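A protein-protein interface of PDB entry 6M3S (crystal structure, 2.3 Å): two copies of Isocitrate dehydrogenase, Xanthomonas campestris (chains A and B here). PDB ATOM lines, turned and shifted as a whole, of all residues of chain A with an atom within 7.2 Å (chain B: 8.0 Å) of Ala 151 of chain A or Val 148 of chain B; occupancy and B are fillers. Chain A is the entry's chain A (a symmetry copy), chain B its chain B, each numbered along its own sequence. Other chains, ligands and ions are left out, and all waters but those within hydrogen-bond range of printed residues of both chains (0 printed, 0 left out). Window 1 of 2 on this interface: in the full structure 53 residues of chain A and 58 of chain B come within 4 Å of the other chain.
Of the printed residues of chain B, Val 153 of chain A touches Val 146 and Ala 147. Of the printed residues of chain B, Ser 188 of chain A touches Gln 138 (3.3 Å), Glu 139 (3.7 Å), Val 140 (3.96 Å), Ala 147 (3.3 Å), Val 148 (2.7 Å) and Ser 149 (3.6 Å). Printed residues of chain B within 4 Å of Thr 189 of chain A: Ala 147, Val 148 and Ser 149. Printed residues of chain A within 4 Å of Gln 138 of chain B: Ile 186 (3.6 Å), Lys 187 (2.8 Å) and Ser 188 (3.3 Å). Of the printed residues of chain A, Ser 149 of chain B touches Gly 150, Ala 151, Ile 186, Ser 188 and Thr 189. The nearest residue of chain A that does not touch Val 148 of chain B is Arg 152 of chain A (4.2 Å).
Ser 149 of chain A touches Gly 150 of chain B, and with the chains exchanged Gly 150 of chain A touches Ser 149 of chain B. Ser 149 of chain A touches Ala 151 of chain B, and with the chains exchanged Ala 151 of chain A touches Ser 149 of chain B. Ser 149 of chain A touches Ile 186 of chain B, and with the chains exchanged Ile 186 of chain A touches Ser 149 of chain B. Of the 23 pairs that touch across the chains among the printed residues, 6 have their exchanged pair printed and touching as well.
The backbone carbonyl oxygen (O) of Glu 139 of chain B is in hydrogen-bond range of the backbone NH (N) of Val 148 of chain B (2.9 Å). The backbone NH (N) of Ser 141 of chain B lies within hydrogen-bond range of the backbone carbonyl oxygen (O) of Val 146 of chain B. N of Gly 131 of chain A is in hydrogen-bond range of O of Arg 152 of chain A. The side-chain carboxylate (OE2) of Glu 136 of chain A lies within salt-bridge range of the guanidinium group (NH1) of Arg 152 of chain A (3.2 Å).
OE1 of Gln 138 of chain B lies within hydrogen-bond range of N of Lys 187 of chain A (2.8 Å). N of Ser 188 of chain A is in hydrogen-bond range of OE1 of Gln 138 of chain B, at 3.3 Å. The backbone carbonyl oxygen (O) of Val 153 of chain A lies within hydrogen-bond range of the backbone NH (N) of Ala 147 of chain B, at 2.7 Å. O of Val 148 of chain B lies within hydrogen-bond range of OG of Ser 188 of chain A, at 2.7 Å. The backbone NH (N) of Ala 151 of chain A is in hydrogen-bond range of the backbone carbonyl oxygen (O) of Ser 149 of chain B, at 2.8 Å. OG1 of Thr 189 of chain A is in hydrogen-bond range of OG of Ser 149 of chain B, at 2.9 Å. The backbone carbonyl oxygen (O) of Ser 149 of chain A lies within hydrogen-bond range of the backbone NH (N) of Ala 151 of chain B (2.7 Å).
Of the 16 printed residues of chain B, 10 touch a printed residue of chain A. Printed residues of chain B that touch a printed residue of chain A: Gln 138, Glu 139, Val 140, Val 146, Ala 147, Val 148, Ser 149, Gly 150, Ala 151 and Ile 186. Among the printed residues, 23 pairs touch across the chains.
Among the printed residues, pairs that only touch across the chains: Ser 149 of chain A with Gly 150 of chain B, Ser 149 of chain A with Ile 186 of chain B, Gly 150 of chain A with Ser 149 of chain B, Ala 151 of chain A with Val 148 of chain B, Arg 152 of chain A with Val 146 of chain B, Arg 152 of chain A with Ala 147 of chain B, Val 153 of chain A with Val 146 of chain B, Ile 186 of chain A with Gln 138 of chain B, Ile 186 of chain A with Ser 149 of chain B, Ser 188 of chain A with Glu 139 of chain B, Ser 188 of chain A with Val 140 of chain B, Ser 188 of chain A with Ala 147 of chain B, Ser 188 of chain A with Ser 149 of chain B, Thr 189 of chain A with Ala 147 of chain B, Thr 189 of chain A with Val 148 of chain B and Leu 192 of chain A with Ala 147 of chain B.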
ATOM      1  N   GLU A 130     -16.610  30.822  -2.076  1.00  0.00           N
ATOM      2  CA  GLU A 130     -17.057  30.676  -0.665  1.00  0.00           C
ATOM      3  C   GLU A 130     -15.861  30.238   0.173  1.00  0.00           C
ATOM      4  O   GLU A 130     -14.754  30.783  -0.041  1.00  0.00           O
ATOM      5  CB  GLU A 130     -18.321  29.794  -0.541  1.00  0.00           C
ATOM      6  CG  GLU A 130     -18.280  28.402  -1.169  1.00  0.00           C
ATOM      7  CD  GLU A 130     -19.519  27.496  -1.014  1.00  0.00           C
ATOM      8  OE1 GLU A 130     -20.660  27.955  -1.234  1.00  0.00           O
ATOM      9  OE2 GLU A 130     -19.353  26.277  -0.730  1.00  0.00           O
ATOM     10  N   GLY A 131     -16.088  29.346   1.131  1.00  0.00           N
ATOM     11  CA  GLY A 131     -15.058  28.909   2.077  1.00  0.00           C
ATOM     12  C   GLY A 131     -14.705  30.012   3.058  1.00  0.00           C
ATOM     13  O   GLY A 131     -15.611  30.680   3.590  1.00  0.00           O
ATOM     14  N   ALA A 132     -13.412  30.186   3.305  1.00  0.00           N
ATOM     15  CA  ALA A 132     -12.884  31.085   4.349  1.00  0.00           C
ATOM     16  C   ALA A 132     -12.629  32.491   3.794  1.00  0.00           C
ATOM     17  O   ALA A 132     -12.301  33.366   4.608  1.00  0.00           O
ATOM     18  CB  ALA A 132     -11.649  30.468   4.930  1.00  0.00           C
ATOM     19  N   TYR A 133     -12.851  32.727   2.492  1.00  0.00           N
ATOM     20  CA  TYR A 133     -12.593  34.028   1.815  1.00  0.00           C
ATOM     21  C   TYR A 133     -13.900  34.826   1.792  1.00  0.00           C
ATOM     22  O   TYR A 133     -14.434  35.191   0.701  1.00  0.00           O
ATOM     23  CB  TYR A 133     -11.958  33.811   0.435  1.00  0.00           C
ATOM     24  CG  TYR A 133     -10.496  33.453   0.496  1.00  0.00           C
ATOM     25  CD1 TYR A 133      -9.922  33.035   1.687  1.00  0.00           C
ATOM     26  CD2 TYR A 133      -9.675  33.564  -0.609  1.00  0.00           C
ATOM     27  CE1 TYR A 133      -8.580  32.729   1.779  1.00  0.00           C
ATOM     28  CE2 TYR A 133      -8.324  33.244  -0.536  1.00  0.00           C
ATOM     29  CZ  TYR A 133      -7.776  32.820   0.657  1.00  0.00           C
ATOM     30  OH  TYR A 133      -6.450  32.506   0.757  1.00  0.00           O
ATOM     31  N   LEU A 134     -14.415  35.079   2.993  1.00  0.00           N
ATOM     32  CA  LEU A 134     -15.717  35.746   3.205  1.00  0.00           C
ATOM     33  C   LEU A 134     -15.488  36.999   4.050  1.00  0.00           C
ATOM     34  O   LEU A 134     -15.080  36.863   5.223  1.00  0.00           O
ATOM     35  CB  LEU A 134     -16.685  34.759   3.865  1.00  0.00           C
ATOM     36  CG  LEU A 134     -17.039  33.541   3.006  1.00  0.00           C
ATOM     37  CD1 LEU A 134     -18.347  32.913   3.454  1.00  0.00           C
ATOM     38  CD2 LEU A 134     -17.121  33.882   1.518  1.00  0.00           C
ATOM     39  N   GLU A 136     -17.951  39.064   5.069  1.00  0.00           N
ATOM     40  CA  GLU A 136     -18.987  39.058   6.133  1.00  0.00           C
ATOM     41  C   GLU A 136     -18.522  38.140   7.277  1.00  0.00           C
ATOM     42  O   GLU A 136     -17.906  37.097   7.013  1.00  0.00           O
ATOM     43  CB  GLU A 136     -20.359  38.694   5.547  1.00  0.00           C
ATOM     44  CG  GLU A 136     -20.428  37.335   4.862  1.00  0.00           C
ATOM     45  CD  GLU A 136     -20.060  37.258   3.382  1.00  0.00           C
ATOM     46  OE1 GLU A 136     -19.107  37.959   2.936  1.00  0.00           O
ATOM     47  OE2 GLU A 136     -20.712  36.467   2.674  1.00  0.00           O
ATOM     48  N   SER A 149     -13.605  35.377  12.740  1.00  0.00           N
ATOM     49  CA  SER A 149     -13.799  35.229  11.283  1.00  0.00           C
ATOM     50  C   SER A 149     -14.541  33.919  11.035  1.00  0.00           C
ATOM     51  O   SER A 149     -14.540  33.041  11.886  1.00  0.00           O
ATOM     52  CB  SER A 149     -12.499  35.287  10.539  1.00  0.00           C
ATOM     53  OG  SER A 149     -11.569  34.401  11.109  1.00  0.00           O
ATOM     54  N   GLY A 150     -15.181  33.830   9.898  1.00  0.00           N
ATOM     55  CA  GLY A 150     -16.095  32.729   9.585  1.00  0.00           C
ATOM     56  C   GLY A 150     -15.779  32.176   8.221  1.00  0.00           C
ATOM     57  O   GLY A 150     -15.155  32.874   7.393  1.00  0.00           O
ATOM     58  N   ALA A 151     -16.203  30.939   8.019  1.00  0.00           N
ATOM     59  CA  ALA A 151     -16.181  30.256   6.723  1.00  0.00           C
ATOM     60  C   ALA A 151     -17.592  29.729   6.470  1.00  0.00           C
ATOM     61  O   ALA A 151     -18.277  29.350   7.437  1.00  0.00           O
ATOM     62  CB  ALA A 151     -15.125  29.175   6.767  1.00  0.00           C
ATOM     63  N   ARG A 152     -18.014  29.742   5.218  1.00  0.00           N
ATOM     64  CA  ARG A 152     -19.310  29.190   4.783  1.00  0.00           C
ATOM     65  C   ARG A 152     -19.034  28.197   3.661  1.00  0.00           C
ATOM     66  O   ARG A 152     -18.296  28.548   2.725  1.00  0.00           O
ATOM     67  CB  ARG A 152     -20.275  30.284   4.318  1.00  0.00           C
ATOM     68  CG  ARG A 152     -21.737  29.853   4.347  1.00  0.00           C
ATOM     69  CD  ARG A 152     -22.739  30.885   3.826  1.00  0.00           C
ATOM     70  NE  ARG A 152     -22.256  31.422   2.560  1.00  0.00           N
ATOM     71  CZ  ARG A 152     -21.741  32.647   2.386  1.00  0.00           C
ATOM     72  NH1 ARG A 152     -21.691  33.499   3.402  1.00  0.00           N
ATOM     73  NH2 ARG A 152     -21.291  33.034   1.198  1.00  0.00           N
ATOM     74  N   VAL A 153     -19.609  27.006   3.776  1.00  0.00           N
ATOM     75  CA  VAL A 153     -19.630  25.996   2.688  1.00  0.00           C
ATOM     76  C   VAL A 153     -21.070  25.499   2.500  1.00  0.00           C
ATOM     77  O   VAL A 153     -21.743  25.212   3.487  1.00  0.00           O
ATOM     78  CB  VAL A 153     -18.639  24.855   2.975  1.00  0.00           C
ATOM     79  CG1 VAL A 153     -18.788  23.720   1.976  1.00  0.00           C
ATOM     80  CG2 VAL A 153     -17.205  25.374   3.000  1.00  0.00           C
ATOM     81  N   ILE A 186     -12.426  20.423  11.268  1.00  0.00           N
ATOM     82  CA  ILE A 186     -13.447  21.402  10.814  1.00  0.00           C
ATOM     83  C   ILE A 186     -14.604  20.606  10.206  1.00  0.00           C
ATOM     84  O   ILE A 186     -14.749  20.587   8.960  1.00  0.00           O
ATOM     85  CB  ILE A 186     -12.795  22.427   9.864  1.00  0.00           C
ATOM     86  CG1 ILE A 186     -11.502  22.965  10.484  1.00  0.00           C
ATOM     87  CG2 ILE A 186     -13.782  23.542   9.532  1.00  0.00           C
ATOM     88  CD1 ILE A 186     -10.813  24.044   9.690  1.00  0.00           C
ATOM     89  N   LYS A 187     -15.400  19.968  11.076  1.00  0.00           N
ATOM     90  CA  LYS A 187     -16.353  18.894  10.689  1.00  0.00           C
ATOM     91  C   LYS A 187     -17.531  19.465   9.905  1.00  0.00           C
ATOM     92  O   LYS A 187     -18.070  18.757   9.034  1.00  0.00           O
ATOM     93  CB  LYS A 187     -16.863  18.145  11.919  1.00  0.00           C
ATOM     94  CG  LYS A 187     -15.798  17.366  12.680  1.00  0.00           C
ATOM     95  CD  LYS A 187     -16.377  16.542  13.796  1.00  0.00           C
ATOM     96  CE  LYS A 187     -15.342  15.935  14.717  1.00  0.00           C
ATOM     97  NZ  LYS A 187     -14.455  14.972  14.011  1.00  0.00           N
ATOM     98  N   SER A 188     -17.940  20.694  10.198  1.00  0.00           N
ATOM     99  CA  SER A 188     -19.127  21.310   9.565  1.00  0.00           C
ATOM    100  C   SER A 188     -18.816  21.658   8.108  1.00  0.00           C
ATOM    101  O   SER A 188     -19.472  21.105   7.217  1.00  0.00           O
ATOM    102  CB  SER A 188     -19.610  22.529  10.350  1.00  0.00           C
ATOM    103  OG  SER A 188     -18.580  23.508  10.567  1.00  0.00           O
ATOM    104  N   THR A 189     -17.880  22.572   7.852  1.00  0.00           N
ATOM    105  CA  THR A 189     -17.679  23.156   6.491  1.00  0.00           C
ATOM    106  C   THR A 189     -16.836  22.214   5.632  1.00  0.00           C
ATOM    107  O   THR A 189     -17.319  21.785   4.565  1.00  0.00           O
ATOM    108  CB  THR A 189     -17.067  24.553   6.557  1.00  0.00           C
ATOM    109  OG1 THR A 189     -16.005  24.514   7.509  1.00  0.00           O
ATOM    110  CG2 THR A 189     -18.103  25.591   6.939  1.00  0.00           C
ATOM    111  N   LEU A 192     -18.801  18.927   5.173  1.00  0.00           N
ATOM    112  CA  LEU A 192     -19.889  19.002   4.156  1.00  0.00           C
ATOM    113  C   LEU A 192     -19.273  18.934   2.750  1.00  0.00           C
ATOM    114  O   LEU A 192     -19.825  18.235   1.880  1.00  0.00           O
ATOM    115  CB  LEU A 192     -20.734  20.271   4.334  1.00  0.00           C
ATOM    116  CG  LEU A 192     -21.756  20.525   3.224  1.00  0.00           C
ATOM    117  CD1 LEU A 192     -22.776  19.388   3.110  1.00  0.00           C
ATOM    118  CD2 LEU A 192     -22.468  21.859   3.420  1.00  0.00           C
ATOM    119  N   ALA B 132      -8.351  28.691  13.862  1.00  0.00           N
ATOM    120  CA  ALA B 132      -9.431  28.004  13.126  1.00  0.00           C
ATOM    121  C   ALA B 132      -9.715  26.628  13.740  1.00  0.00           C
ATOM    122  O   ALA B 132     -10.666  26.004  13.297  1.00  0.00           O
ATOM    123  CB  ALA B 132      -9.081  27.896  11.664  1.00  0.00           C
ATOM    124  N   SER B 135     -13.728  23.841  18.037  1.00  0.00           N
ATOM    125  CA  SER B 135     -14.927  22.963  17.982  1.00  0.00           C
ATOM    126  C   SER B 135     -16.226  23.783  18.083  1.00  0.00           C
ATOM    127  O   SER B 135     -17.263  23.324  17.546  1.00  0.00           O
ATOM    128  CB  SER B 135     -14.857  21.929  19.067  1.00  0.00           C
ATOM    129  OG  SER B 135     -16.066  21.919  19.797  1.00  0.00           O
ATOM    130  N   GLU B 136     -16.192  24.936  18.764  1.00  0.00           N
ATOM    131  CA  GLU B 136     -17.388  25.793  18.989  1.00  0.00           C
ATOM    132  C   GLU B 136     -17.648  26.609  17.719  1.00  0.00           C
ATOM    133  O   GLU B 136     -16.681  26.954  17.011  1.00  0.00           O
ATOM    134  CB  GLU B 136     -17.246  26.677  20.241  1.00  0.00           C
ATOM    135  CG  GLU B 136     -15.937  27.455  20.353  1.00  0.00           C
ATOM    136  CD  GLU B 136     -14.752  26.756  21.024  1.00  0.00           C
ATOM    137  OE1 GLU B 136     -14.836  25.534  21.315  1.00  0.00           O
ATOM    138  OE2 GLU B 136     -13.722  27.435  21.255  1.00  0.00           O
ATOM    139  N   GLY B 137     -18.914  26.903  17.435  1.00  0.00           N
ATOM    140  CA  GLY B 137     -19.313  27.692  16.257  1.00  0.00           C
ATOM    141  C   GLY B 137     -19.412  26.865  14.975  1.00  0.00           C
ATOM    142  O   GLY B 137     -19.708  27.467  13.929  1.00  0.00           O
ATOM    143  N   GLN B 138     -19.171  25.547  15.024  1.00  0.00           N
ATOM    144  CA  GLN B 138     -19.362  24.616  13.879  1.00  0.00           C
ATOM    145  C   GLN B 138     -20.826  24.185  13.832  1.00  0.00           C
ATOM    146  O   GLN B 138     -21.275  23.568  14.792  1.00  0.00           O
ATOM    147  CB  GLN B 138     -18.471  23.379  13.991  1.00  0.00           C
ATOM    148  CG  GLN B 138     -16.986  23.682  13.844  1.00  0.00           C
ATOM    149  CD  GLN B 138     -16.171  22.417  13.706  1.00  0.00           C
ATOM    150  OE1 GLN B 138     -16.607  21.452  13.086  1.00  0.00           O
ATOM    151  NE2 GLN B 138     -14.966  22.423  14.249  1.00  0.00           N
ATOM    152  N   GLU B 139     -21.537  24.526  12.760  1.00  0.00           N
ATOM    153  CA  GLU B 139     -22.995  24.279  12.613  1.00  0.00           C
ATOM    154  C   GLU B 139     -23.320  23.955  11.159  1.00  0.00           C
ATOM    155  O   GLU B 139     -22.694  24.536  10.249  1.00  0.00           O
ATOM    156  CB  GLU B 139     -23.826  25.490  13.042  1.00  0.00           C
ATOM    157  CG  GLU B 139     -23.765  25.758  14.537  1.00  0.00           C
ATOM    158  CD  GLU B 139     -24.652  26.905  14.996  1.00  0.00           C
ATOM    159  OE1 GLU B 139     -24.753  27.129  16.225  1.00  0.00           O
ATOM    160  OE2 GLU B 139     -25.246  27.571  14.121  1.00  0.00           O
ATOM    161  N   VAL B 140     -24.277  23.053  10.978  1.00  0.00           N
ATOM    162  CA  VAL B 140     -24.875  22.696   9.660  1.00  0.00           C
ATOM    163  C   VAL B 140     -26.369  22.991   9.764  1.00  0.00           C
ATOM    164  O   VAL B 140     -26.955  22.614  10.772  1.00  0.00           O
ATOM    165  CB  VAL B 140     -24.589  21.221   9.310  1.00  0.00           C
ATOM    166  CG1 VAL B 140     -25.117  20.863   7.928  1.00  0.00           C
ATOM    167  CG2 VAL B 140     -23.099  20.905   9.402  1.00  0.00           C
ATOM    168  N   SER B 141     -26.952  23.679   8.784  1.00  0.00           N
ATOM    169  CA  SER B 141     -28.401  24.011   8.765  1.00  0.00           C
ATOM    170  C   SER B 141     -29.187  22.701   8.753  1.00  0.00           C
ATOM    171  O   SER B 141     -28.613  21.670   8.366  1.00  0.00           O
ATOM    172  CB  SER B 141     -28.759  24.882   7.607  1.00  0.00           C
ATOM    173  OG  SER B 141     -28.499  24.228   6.382  1.00  0.00           O
ATOM    174  N   GLU B 145     -27.904  22.019   3.815  1.00  0.00           N
ATOM    175  CA  GLU B 145     -27.519  22.859   2.648  1.00  0.00           C
ATOM    176  C   GLU B 145     -26.376  23.829   2.982  1.00  0.00           C
ATOM    177  O   GLU B 145     -25.615  24.163   2.092  1.00  0.00           O
ATOM    178  CB  GLU B 145     -28.722  23.660   2.158  1.00  0.00           C
ATOM    179  CG  GLU B 145     -28.667  23.935   0.677  1.00  0.00           C
ATOM    180  CD  GLU B 145     -29.241  22.806  -0.160  1.00  0.00           C
ATOM    181  OE1 GLU B 145     -28.700  21.673  -0.123  1.00  0.00           O
ATOM    182  OE2 GLU B 145     -30.244  23.058  -0.830  1.00  0.00           O
ATOM    183  N   VAL B 146     -26.257  24.296   4.218  1.00  0.00           N
ATOM    184  CA  VAL B 146     -25.298  25.386   4.554  1.00  0.00           C
ATOM    185  C   VAL B 146     -24.546  25.034   5.837  1.00  0.00           C
ATOM    186  O   VAL B 146     -25.177  24.809   6.870  1.00  0.00           O
ATOM    187  CB  VAL B 146     -26.016  26.743   4.662  1.00  0.00           C
ATOM    188  CG1 VAL B 146     -25.029  27.876   4.893  1.00  0.00           C
ATOM    189  CG2 VAL B 146     -26.848  27.025   3.428  1.00  0.00           C
ATOM    190  N   ALA B 147     -23.226  25.010   5.768  1.00  0.00           N
ATOM    191  CA  ALA B 147     -22.385  24.816   6.953  1.00  0.00           C
ATOM    192  C   ALA B 147     -21.630  26.108   7.205  1.00  0.00           C
ATOM    193  O   ALA B 147     -21.234  26.778   6.239  1.00  0.00           O
ATOM    194  CB  ALA B 147     -21.450  23.667   6.742  1.00  0.00           C
ATOM    195  N   VAL B 148     -21.417  26.398   8.478  1.00  0.00           N
ATOM    196  CA  VAL B 148     -20.540  27.500   8.947  1.00  0.00           C
ATOM    197  C   VAL B 148     -19.543  26.915   9.947  1.00  0.00           C
ATOM    198  O   VAL B 148     -19.844  25.917  10.581  1.00  0.00           O
ATOM    199  CB  VAL B 148     -21.336  28.670   9.559  1.00  0.00           C
ATOM    200  CG1 VAL B 148     -22.139  29.386   8.487  1.00  0.00           C
ATOM    201  CG2 VAL B 148     -22.243  28.196  10.687  1.00  0.00           C
ATOM    202  N   SER B 149     -18.383  27.554  10.024  1.00  0.00           N
ATOM    203  CA  SER B 149     -17.328  27.317  11.025  1.00  0.00           C
ATOM    204  C   SER B 149     -16.671  28.677  11.262  1.00  0.00           C
ATOM    205  O   SER B 149     -16.841  29.577  10.414  1.00  0.00           O
ATOM    206  CB  SER B 149     -16.345  26.270  10.548  1.00  0.00           C
ATOM    207  OG  SER B 149     -15.641  26.741   9.398  1.00  0.00           O
ATOM    208  N   GLY B 150     -15.970  28.818  12.373  1.00  0.00           N
ATOM    209  CA  GLY B 150     -15.430  30.114  12.806  1.00  0.00           C
ATOM    210  C   GLY B 150     -13.990  29.984  13.239  1.00  0.00           C
ATOM    211  O   GLY B 150     -13.496  28.844  13.399  1.00  0.00           O
ATOM    212  N   ALA B 151     -13.324  31.121  13.373  1.00  0.00           N
ATOM    213  CA  ALA B 151     -11.974  31.226  13.955  1.00  0.00           C
ATOM    214  C   ALA B 151     -11.968  32.377  14.968  1.00  0.00           C
ATOM    215  O   ALA B 151     -12.753  33.312  14.825  1.00  0.00           O
ATOM    216  CB  ALA B 151     -10.965  31.371  12.854  1.00  0.00           C
ATOM    217  N   ILE B 186      -8.200  37.828   5.397  1.00  0.00           N
ATOM    218  CA  ILE B 186      -8.826  37.546   6.716  1.00  0.00           C
ATOM    219  C   ILE B 186      -8.273  38.612   7.661  1.00  0.00           C
ATOM    220  O   ILE B 186      -7.257  38.357   8.363  1.00  0.00           O
ATOM    221  CB  ILE B 186      -8.581  36.090   7.146  1.00  0.00           C
ATOM    222  CG1 ILE B 186      -8.934  35.138   6.005  1.00  0.00           C
ATOM    223  CG2 ILE B 186      -9.351  35.753   8.412  1.00  0.00           C
ATOM    224  CD1 ILE B 186      -8.687  33.680   6.308  1.00  0.00           C
